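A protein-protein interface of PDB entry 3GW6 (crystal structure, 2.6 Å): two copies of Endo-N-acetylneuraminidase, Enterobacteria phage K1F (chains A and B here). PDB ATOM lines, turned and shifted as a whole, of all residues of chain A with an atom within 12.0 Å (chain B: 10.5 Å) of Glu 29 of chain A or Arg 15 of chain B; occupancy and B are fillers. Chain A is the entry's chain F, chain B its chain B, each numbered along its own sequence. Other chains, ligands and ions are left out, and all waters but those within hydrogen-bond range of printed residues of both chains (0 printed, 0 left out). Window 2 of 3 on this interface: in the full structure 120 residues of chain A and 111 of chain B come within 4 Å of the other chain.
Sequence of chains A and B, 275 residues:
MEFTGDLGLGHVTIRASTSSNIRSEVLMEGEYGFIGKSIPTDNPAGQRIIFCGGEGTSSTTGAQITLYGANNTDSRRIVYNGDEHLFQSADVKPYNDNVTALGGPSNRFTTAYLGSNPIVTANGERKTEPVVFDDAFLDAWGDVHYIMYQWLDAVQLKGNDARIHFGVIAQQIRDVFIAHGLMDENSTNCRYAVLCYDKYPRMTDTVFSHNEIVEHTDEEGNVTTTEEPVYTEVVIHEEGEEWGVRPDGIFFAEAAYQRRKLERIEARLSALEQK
Met 28 of chain A touches just these residues of chain B: Ile 14 (3.5 Å) and Ser 24 (3.1 Å).
Of chain B, only Ile 14 (3.0 Å), Arg 15 (3.1 Å) and Ser 24 (2.9 Å) come within 4 Å of Glu 29 of chain A.
Of the printed residues of chain B, Gly 30 of chain A touches Ile 22 (3.5 Å).
Of the printed residues of chain B, Glu 31 of chain A touches Ile 22 (2.6 Å).
Printed residues of chain B within 4 Å of Tyr 32 of chain A: Ile 22 (3.4 Å), Arg 23 (3.2 Å) and Ser 24 (3.1 Å).
Printed residues of chain B within 4 Å of Phe 34 of chain A: Ser 24, Glu 25 and Val 26.
Of chain A, only Leu 27 (3.0 Å) comes within 4 Å of Thr 13 of chain B.
Printed residues of chain A within 4 Å of Arg 15 of chain B: Glu 29.
Of the printed residues of chain A, Arg 23 of chain B touches Tyr 32 (3.2 Å).
Cys 52 of chain B touches none of the printed residues of chain A.
Gly 53 of chain B touches none of the printed residues of chain A.
The nearest residue of chain B that does not touch Glu 29 of chain A is Thr 13 of chain B (4.2 Å).
The nearest residue of chain A that does not touch Arg 15 of chain B is Leu 27 of chain A (5.2 Å).
The nearest printed residue of chain B that does not touch Phe 34 of chain A is Leu 27 of chain B (4.3 Å).
NH2 of Arg 23 of chain B lies within salt-bridge range of OE1 of Glu 25 of chain B (2.9 Å).
Val 26 of chain A touches Ile 14 of chain B, but with the chains exchanged Ile 14 of chain A does not touch Val 26 of chain B (8.8 Å).
Leu 27 of chain A touches Ile 14 of chain B, but with the chains exchanged Ile 14 of chain A does not touch Leu 27 of chain B (12.2 Å).
The backbone NH (N) of Leu 27 of chain A is in hydrogen-bond range of the backbone carbonyl oxygen (O) of Val 12 of chain B (2.9 Å).
The backbone carbonyl oxygen (O) of Ile 14 of chain B sits at hydrogen-bond distance from the backbone NH (N) of Glu 29 of chain A (3.0 Å).
The backbone carbonyl oxygen (O) of Ile 22 of chain B is in hydrogen-bond range of the backbone NH (N) of Tyr 32 of chain A, at 3.4 Å.
O of Phe 34 of chain A lies within hydrogen-bond range of N of Val 26 of chain B (2.8 Å).
N of Glu 31 of chain A lies within hydrogen-bond range of O of Ile 22 of chain B, at 2.6 Å.
The backbone carbonyl oxygen of Leu 27 of chain A lies within hydrogen-bond range of the backbone NH of Ile 14 of chain B.
OG of Ser 24 of chain B is in hydrogen-bond range of O of Glu 29 of chain A (2.9 Å).
O of Ser 24 of chain B lies within hydrogen-bond range of N of Phe 34 of chain A (2.7 Å).
N of Ser 24 of chain B sits at hydrogen-bond distance from O of Tyr 32 of chain A (3.1 Å).
The backbone carbonyl oxygen (O) of Glu 25 of chain A lies within hydrogen-bond range of the backbone NH (N) of Val 12 of chain B (3.0 Å).
Printed residues of chain B that touch a printed residue of chain A: Val 12, Thr 13, Ile 14, Arg 15, Ile 22, Arg 23, Ser 24, Glu 25, Val 26 and Glu 55.
Hydrophobic or aromatic side chains of chain B that line the printed part of chain A: Val 12 and Ile 14.
Along chain B the printed residues that touch a printed residue of chain A span positions 12 to 55.
Printed residues of chain A that touch a printed residue of chain B: Ile 14, Glu 25, Val 26, Leu 27, Met 28, Glu 29, Gly 30, Glu 31, Tyr 32, Gly 33, Phe 34 and Ile 35.
Among the printed residues, 23 pairs touch across the chains.
Among the printed residues, no Asp or Glu carboxylate lies within 4 Å of a Lys or Arg side-chain nitrogen of the other chain.
CG1 of Val 12 of chain B touches CD1 of Ile 14 of chain A, 3.6 Å away.
Ile 14 of chain B touches Val 26 of chain A (CG1 to CG1, 3.9 Å).
Leu 27 of chain A touches Thr 13 of chain B.
Ser 24 of chain B touches Met 28 of chain A.
OE1 of Glu 29 of chain A touches CG of Arg 15 of chain B (3.1 Å).
Ile 22 of chain B touches Gly 30 of chain A (O to C, 3.5 Å).
O of Tyr 32 of chain A touches CA of Arg 23 of chain B (3.2 Å).
O of Ser 24 of chain B touches CA of Gly 33 of chain A (3.5 Å).
Phe 34 of chain A touches Glu 25 of chain B.
Val 26 of chain B touches Ile 35 of chain A.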
ATOM      1  N   ILE A  14      19.449 -17.135   4.559  1.00  0.00           N
ATOM      2  CA  ILE A  14      19.868 -17.751   5.807  1.00  0.00           C
ATOM      3  C   ILE A  14      19.745 -19.261   5.678  1.00  0.00           C
ATOM      4  O   ILE A  14      18.712 -19.775   5.244  1.00  0.00           O
ATOM      5  CB  ILE A  14      19.012 -17.270   7.000  1.00  0.00           C
ATOM      6  CG1 ILE A  14      18.974 -15.742   7.058  1.00  0.00           C
ATOM      7  CG2 ILE A  14      19.545 -17.848   8.305  1.00  0.00           C
ATOM      8  CD1 ILE A  14      20.339 -15.100   7.069  1.00  0.00           C
ATOM      9  N   GLU A  25      17.944 -19.835  11.290  1.00  0.00           N
ATOM     10  CA  GLU A  25      17.693 -19.019  12.469  1.00  0.00           C
ATOM     11  C   GLU A  25      18.378 -17.664  12.413  1.00  0.00           C
ATOM     12  O   GLU A  25      19.589 -17.577  12.221  1.00  0.00           O
ATOM     13  CB  GLU A  25      18.143 -19.752  13.733  1.00  0.00           C
ATOM     14  CG  GLU A  25      17.177 -20.809  14.231  1.00  0.00           C
ATOM     15  CD  GLU A  25      17.774 -21.667  15.328  1.00  0.00           C
ATOM     16  OE1 GLU A  25      18.965 -22.030  15.218  1.00  0.00           O
ATOM     17  OE2 GLU A  25      17.052 -21.980  16.298  1.00  0.00           O
ATOM     18  N   VAL A  26      17.587 -16.611  12.580  1.00  0.00           N
ATOM     19  CA  VAL A  26      18.122 -15.288  12.850  1.00  0.00           C
ATOM     20  C   VAL A  26      17.865 -14.985  14.323  1.00  0.00           C
ATOM     21  O   VAL A  26      16.756 -15.182  14.818  1.00  0.00           O
ATOM     22  CB  VAL A  26      17.444 -14.217  11.993  1.00  0.00           C
ATOM     23  CG1 VAL A  26      17.984 -12.838  12.345  1.00  0.00           C
ATOM     24  CG2 VAL A  26      17.642 -14.520  10.516  1.00  0.00           C
ATOM     25  N   LEU A  27      18.888 -14.524  15.032  1.00  0.00           N
ATOM     26  CA  LEU A  27      18.734 -14.231  16.451  1.00  0.00           C
ATOM     27  C   LEU A  27      19.238 -12.843  16.795  1.00  0.00           C
ATOM     28  O   LEU A  27      20.379 -12.493  16.505  1.00  0.00           O
ATOM     29  CB  LEU A  27      19.414 -15.295  17.312  1.00  0.00           C
ATOM     30  CG  LEU A  27      18.474 -16.437  17.703  1.00  0.00           C
ATOM     31  CD1 LEU A  27      19.222 -17.744  17.935  1.00  0.00           C
ATOM     32  CD2 LEU A  27      17.632 -16.053  18.924  1.00  0.00           C
ATOM     33  N   MET A  28      18.369 -12.055  17.418  1.00  0.00           N
ATOM     34  CA  MET A  28      18.678 -10.672  17.734  1.00  0.00           C
ATOM     35  C   MET A  28      19.044 -10.528  19.206  1.00  0.00           C
ATOM     36  O   MET A  28      18.338 -11.028  20.084  1.00  0.00           O
ATOM     37  CB  MET A  28      17.484  -9.786  17.385  1.00  0.00           C
ATOM     38  CG  MET A  28      16.788 -10.207  16.105  1.00  0.00           C
ATOM     39  SD  MET A  28      16.245  -8.813  15.111  1.00  0.00           S
ATOM     40  CE  MET A  28      17.767  -7.878  14.998  1.00  0.00           C
ATOM     41  N   GLU A  29      20.155  -9.848  19.468  1.00  0.00           N
ATOM     42  CA  GLU A  29      20.625  -9.642  20.831  1.00  0.00           C
ATOM     43  C   GLU A  29      20.212  -8.281  21.375  1.00  0.00           C
ATOM     44  O   GLU A  29      19.341  -7.609  20.816  1.00  0.00           O
ATOM     45  CB  GLU A  29      22.143  -9.789  20.906  1.00  0.00           C
ATOM     46  CG  GLU A  29      22.637 -11.220  20.789  1.00  0.00           C
ATOM     47  CD  GLU A  29      24.150 -11.306  20.818  1.00  0.00           C
ATOM     48  OE1 GLU A  29      24.799 -10.235  20.822  1.00  0.00           O
ATOM     49  OE2 GLU A  29      24.687 -12.436  20.839  1.00  0.00           O
ATOM     50  N   GLY A  30      20.846  -7.883  22.473  1.00  0.00           N
ATOM     51  CA  GLY A  30      20.518  -6.638  23.138  1.00  0.00           C
ATOM     52  C   GLY A  30      19.214  -6.768  23.895  1.00  0.00           C
ATOM     53  O   GLY A  30      18.666  -7.862  24.018  1.00  0.00           O
ATOM     54  N   GLU A  31      18.715  -5.651  24.407  1.00  0.00           N
ATOM     55  CA  GLU A  31      17.447  -5.649  25.117  1.00  0.00           C
ATOM     56  C   GLU A  31      16.312  -5.994  24.160  1.00  0.00           C
ATOM     57  O   GLU A  31      15.490  -6.862  24.448  1.00  0.00           O
ATOM     58  CB  GLU A  31      17.196  -4.291  25.773  1.00  0.00           C
ATOM     59  CG  GLU A  31      15.934  -4.248  26.614  1.00  0.00           C
ATOM     60  CD  GLU A  31      15.576  -2.843  27.047  1.00  0.00           C
ATOM     61  OE1 GLU A  31      16.448  -2.151  27.614  1.00  0.00           O
ATOM     62  OE2 GLU A  31      14.420  -2.431  26.818  1.00  0.00           O
ATOM     63  N   TYR A  32      16.274  -5.313  23.019  1.00  0.00           N
ATOM     64  CA  TYR A  32      15.265  -5.585  22.000  1.00  0.00           C
ATOM     65  C   TYR A  32      15.848  -5.603  20.588  1.00  0.00           C
ATOM     66  O   TYR A  32      16.939  -5.086  20.339  1.00  0.00           O
ATOM     67  CB  TYR A  32      14.117  -4.575  22.087  1.00  0.00           C
ATOM     68  CG  TYR A  32      14.516  -3.140  21.832  1.00  0.00           C
ATOM     69  CD1 TYR A  32      14.270  -2.537  20.604  1.00  0.00           C
ATOM     70  CD2 TYR A  32      15.128  -2.383  22.823  1.00  0.00           C
ATOM     71  CE1 TYR A  32      14.629  -1.222  20.370  1.00  0.00           C
ATOM     72  CE2 TYR A  32      15.490  -1.068  22.595  1.00  0.00           C
ATOM     73  CZ  TYR A  32      15.239  -0.494  21.370  1.00  0.00           C
ATOM     74  OH  TYR A  32      15.600   0.816  21.141  1.00  0.00           O
ATOM     75  N   GLY A  33      15.112  -6.205  19.662  1.00  0.00           N
ATOM     76  CA  GLY A  33      15.526  -6.230  18.274  1.00  0.00           C
ATOM     77  C   GLY A  33      14.606  -5.378  17.427  1.00  0.00           C
ATOM     78  O   GLY A  33      13.398  -5.356  17.646  1.00  0.00           O
ATOM     79  N   PHE A  34      15.182  -4.668  16.464  1.00  0.00           N
ATOM     80  CA  PHE A  34      14.407  -3.853  15.542  1.00  0.00           C
ATOM     81  C   PHE A  34      14.642  -4.305  14.106  1.00  0.00           C
ATOM     82  O   PHE A  34      15.782  -4.436  13.663  1.00  0.00           O
ATOM     83  CB  PHE A  34      14.771  -2.379  15.703  1.00  0.00           C
ATOM     84  CG  PHE A  34      14.062  -1.468  14.743  1.00  0.00           C
ATOM     85  CD1 PHE A  34      12.817  -0.949  15.053  1.00  0.00           C
ATOM     86  CD2 PHE A  34      14.648  -1.121  13.539  1.00  0.00           C
ATOM     87  CE1 PHE A  34      12.168  -0.106  14.177  1.00  0.00           C
ATOM     88  CE2 PHE A  34      14.003  -0.275  12.659  1.00  0.00           C
ATOM     89  CZ  PHE A  34      12.763   0.232  12.977  1.00  0.00           C
ATOM     90  N   ILE A  35      13.553  -4.559  13.388  1.00  0.00           N
ATOM     91  CA  ILE A  35      13.622  -4.903  11.974  1.00  0.00           C
ATOM     92  C   ILE A  35      12.751  -3.936  11.178  1.00  0.00           C
ATOM     93  O   ILE A  35      11.524  -4.035  11.198  1.00  0.00           O
ATOM     94  CB  ILE A  35      13.168  -6.352  11.719  1.00  0.00           C
ATOM     95  CG1 ILE A  35      14.149  -7.334  12.359  1.00  0.00           C
ATOM     96  CG2 ILE A  35      13.057  -6.630  10.231  1.00  0.00           C
ATOM     97  CD1 ILE A  35      13.879  -8.777  12.014  1.00  0.00           C
ATOM     98  N   VAL B  12      22.539 -17.084  12.042  1.00  0.00           N
ATOM     99  CA  VAL B  12      23.122 -15.758  12.180  1.00  0.00           C
ATOM    100  C   VAL B  12      22.545 -15.062  13.401  1.00  0.00           C
ATOM    101  O   VAL B  12      21.377 -15.252  13.730  1.00  0.00           O
ATOM    102  CB  VAL B  12      22.848 -14.898  10.936  1.00  0.00           C
ATOM    103  CG1 VAL B  12      21.397 -15.028  10.520  1.00  0.00           C
ATOM    104  CG2 VAL B  12      23.185 -13.447  11.209  1.00  0.00           C
ATOM    105  N   THR B  13      23.364 -14.268  14.083  1.00  0.00           N
ATOM    106  CA  THR B  13      22.852 -13.424  15.153  1.00  0.00           C
ATOM    107  C   THR B  13      23.175 -11.959  14.891  1.00  0.00           C
ATOM    108  O   THR B  13      24.323 -11.598  14.627  1.00  0.00           O
ATOM    109  CB  THR B  13      23.391 -13.823  16.547  1.00  0.00           C
ATOM    110  OG1 THR B  13      24.699 -13.274  16.740  1.00  0.00           O
ATOM    111  CG2 THR B  13      23.429 -15.334  16.706  1.00  0.00           C
ATOM    112  N   ILE B  14      22.141 -11.126  14.948  1.00  0.00           N
ATOM    113  CA  ILE B  14      22.299  -9.689  14.817  1.00  0.00           C
ATOM    114  C   ILE B  14      22.638  -9.122  16.184  1.00  0.00           C
ATOM    115  O   ILE B  14      21.807  -9.140  17.094  1.00  0.00           O
ATOM    116  CB  ILE B  14      21.001  -9.023  14.332  1.00  0.00           C
ATOM    117  CG1 ILE B  14      20.359  -9.835  13.206  1.00  0.00           C
ATOM    118  CG2 ILE B  14      21.263  -7.587  13.898  1.00  0.00           C
ATOM    119  CD1 ILE B  14      21.168  -9.853  11.930  1.00  0.00           C
ATOM    120  N   ARG B  15      23.859  -8.628  16.339  1.00  0.00           N
ATOM    121  CA  ARG B  15      24.277  -8.075  17.620  1.00  0.00           C
ATOM    122  C   ARG B  15      23.958  -6.585  17.699  1.00  0.00           C
ATOM    123  O   ARG B  15      23.643  -5.956  16.687  1.00  0.00           O
ATOM    124  CB  ARG B  15      25.766  -8.320  17.851  1.00  0.00           C
ATOM    125  CG  ARG B  15      26.133  -9.769  18.110  1.00  0.00           C
ATOM    126  CD  ARG B  15      27.635  -9.918  18.261  1.00  0.00           C
ATOM    127  NE  ARG B  15      28.336  -9.617  17.015  1.00  0.00           N
ATOM    128  CZ  ARG B  15      29.646  -9.417  16.929  1.00  0.00           C
ATOM    129  NH1 ARG B  15      30.398  -9.472  18.020  1.00  0.00           N
ATOM    130  NH2 ARG B  15      30.204  -9.148  15.756  1.00  0.00           N
ATOM    131  N   ALA B  16      24.036  -6.029  18.905  1.00  0.00           N
ATOM    132  CA  ALA B  16      23.717  -4.623  19.128  1.00  0.00           C
ATOM    133  C   ALA B  16      24.845  -3.707  18.665  1.00  0.00           C
ATOM    134  O   ALA B  16      24.626  -2.786  17.876  1.00  0.00           O
ATOM    135  CB  ALA B  16      23.401  -4.377  20.599  1.00  0.00           C
ATOM    136  N   ILE B  22      22.426  -2.454  23.507  1.00  0.00           N
ATOM    137  CA  ILE B  22      21.051  -2.235  23.943  1.00  0.00           C
ATOM    138  C   ILE B  22      20.037  -2.781  22.936  1.00  0.00           C
ATOM    139  O   ILE B  22      19.016  -3.349  23.322  1.00  0.00           O
ATOM    140  CB  ILE B  22      20.762  -0.743  24.198  1.00  0.00           C
ATOM    141  CG1 ILE B  22      19.287  -0.534  24.552  1.00  0.00           C
ATOM    142  CG2 ILE B  22      21.144   0.097  22.987  1.00  0.00           C
ATOM    143  CD1 ILE B  22      18.894   0.921  24.688  1.00  0.00           C
ATOM    144  N   ARG B  23      20.316  -2.608  21.648  1.00  0.00           N
ATOM    145  CA  ARG B  23      19.401  -3.077  20.612  1.00  0.00           C
ATOM    146  C   ARG B  23      20.116  -3.540  19.347  1.00  0.00           C
ATOM    147  O   ARG B  23      21.124  -2.963  18.944  1.00  0.00           O
ATOM    148  CB  ARG B  23      18.379  -1.992  20.258  1.00  0.00           C
ATOM    149  CG  ARG B  23      18.985  -0.685  19.774  1.00  0.00           C
ATOM    150  CD  ARG B  23      18.042   0.027  18.812  1.00  0.00           C
ATOM    151  NE  ARG B  23      18.306   1.460  18.731  1.00  0.00           N
ATOM    152  CZ  ARG B  23      17.832   2.253  17.776  1.00  0.00           C
ATOM    153  NH1 ARG B  23      18.119   3.549  17.781  1.00  0.00           N
ATOM    154  NH2 ARG B  23      17.076   1.749  16.807  1.00  0.00           N
ATOM    155  N   SER B  24      19.582  -4.590  18.732  1.00  0.00           N
ATOM    156  CA  SER B  24      20.053  -5.063  17.441  1.00  0.00           C
ATOM    157  C   SER B  24      19.131  -4.529  16.347  1.00  0.00           C
ATOM    158  O   SER B  24      17.918  -4.431  16.542  1.00  0.00           O
ATOM    159  CB  SER B  24      20.089  -6.593  17.416  1.00  0.00           C
ATOM    160  OG  SER B  24      18.914  -7.149  17.983  1.00  0.00           O
ATOM    161  N   GLU B  25      19.709  -4.174  15.204  1.00  0.00           N
ATOM    162  CA  GLU B  25      18.942  -3.571  14.120  1.00  0.00           C
ATOM    163  C   GLU B  25      19.193  -4.238  12.774  1.00  0.00           C
ATOM    164  O   GLU B  25      20.335  -4.408  12.351  1.00  0.00           O
ATOM    165  CB  GLU B  25      19.265  -2.082  13.991  1.00  0.00           C
ATOM    166  CG  GLU B  25      19.042  -1.257  15.243  1.00  0.00           C
ATOM    167  CD  GLU B  25      19.404   0.201  15.030  1.00  0.00           C
ATOM    168  OE1 GLU B  25      19.743   0.889  16.017  1.00  0.00           O
ATOM    169  OE2 GLU B  25      19.353   0.654  13.867  1.00  0.00           O
ATOM    170  N   VAL B  26      18.110  -4.612  12.102  1.00  0.00           N
ATOM    171  CA  VAL B  26      18.174  -4.986  10.697  1.00  0.00           C
ATOM    172  C   VAL B  26      17.380  -3.963   9.893  1.00  0.00           C
ATOM    173  O   VAL B  26      16.171  -3.819  10.079  1.00  0.00           O
ATOM    174  CB  VAL B  26      17.591  -6.376  10.442  1.00  0.00           C
ATOM    175  CG1 VAL B  26      17.416  -6.604   8.947  1.00  0.00           C
ATOM    176  CG2 VAL B  26      18.478  -7.445  11.055  1.00  0.00           C
ATOM    177  N   LEU B  27      18.061  -3.241   9.010  1.00  0.00           N
ATOM    178  CA  LEU B  27      17.398  -2.227   8.201  1.00  0.00           C
ATOM    179  C   LEU B  27      17.392  -2.613   6.729  1.00  0.00           C
ATOM    180  O   LEU B  27      18.438  -2.872   6.138  1.00  0.00           O
ATOM    181  CB  LEU B  27      18.043  -0.856   8.416  1.00  0.00           C
ATOM    182  CG  LEU B  27      17.451  -0.081   9.597  1.00  0.00           C
ATOM    183  CD1 LEU B  27      18.499   0.766  10.313  1.00  0.00           C
ATOM    184  CD2 LEU B  27      16.267   0.770   9.144  1.00  0.00           C
ATOM    185  N   CYS B  52       9.219 -14.561  16.671  1.00  0.00           N
ATOM    186  CA  CYS B  52       9.095 -14.765  18.107  1.00  0.00           C
ATOM    187  C   CYS B  52       9.760 -13.657  18.919  1.00  0.00           C
ATOM    188  O   CYS B  52      10.843 -13.186  18.576  1.00  0.00           O
ATOM    189  CB  CYS B  52       9.685 -16.126  18.492  1.00  0.00           C
ATOM    190  SG  CYS B  52       9.516 -16.547  20.238  1.00  0.00           S
ATOM    191  N   GLY B  53       9.103 -13.249  20.000  1.00  0.00           N
ATOM    192  CA  GLY B  53       9.643 -12.234  20.885  1.00  0.00           C
ATOM    193  C   GLY B  53      10.652 -12.804  21.860  1.00  0.00           C
ATOM    194  O   GLY B  53      11.333 -12.065  22.571  1.00  0.00           O
ATOM    195  N   GLY B  54      10.754 -14.129  21.888  1.00  0.00           N
ATOM    196  CA  GLY B  54      11.657 -14.801  22.801  1.00  0.00           C
ATOM    197  C   GLY B  54      12.822 -15.511  22.138  1.00  0.00           C
ATOM    198  O   GLY B  54      13.051 -15.379  20.936  1.00  0.00           O
ATOM    199  N   GLU B  55      13.553 -16.280  22.939  1.00  0.00           N
ATOM    200  CA  GLU B  55      14.780 -16.937  22.506  1.00  0.00           C
ATOM    201  C   GLU B  55      14.537 -18.216  21.719  1.00  0.00           C
ATOM    202  O   GLU B  55      15.371 -18.618  20.911  1.00  0.00           O
ATOM    203  CB  GLU B  55      15.634 -17.288  23.724  1.00  0.00           C
ATOM    204  CG  GLU B  55      15.047 -18.428  24.554  1.00  0.00           C
ATOM    205  CD  GLU B  55      16.044 -19.039  25.521  1.00  0.00           C
ATOM    206  OE1 GLU B  55      17.208 -18.584  25.548  1.00  0.00           O
ATOM    207  OE2 GLU B  55      15.661 -19.978  26.253  1.00  0.00           O
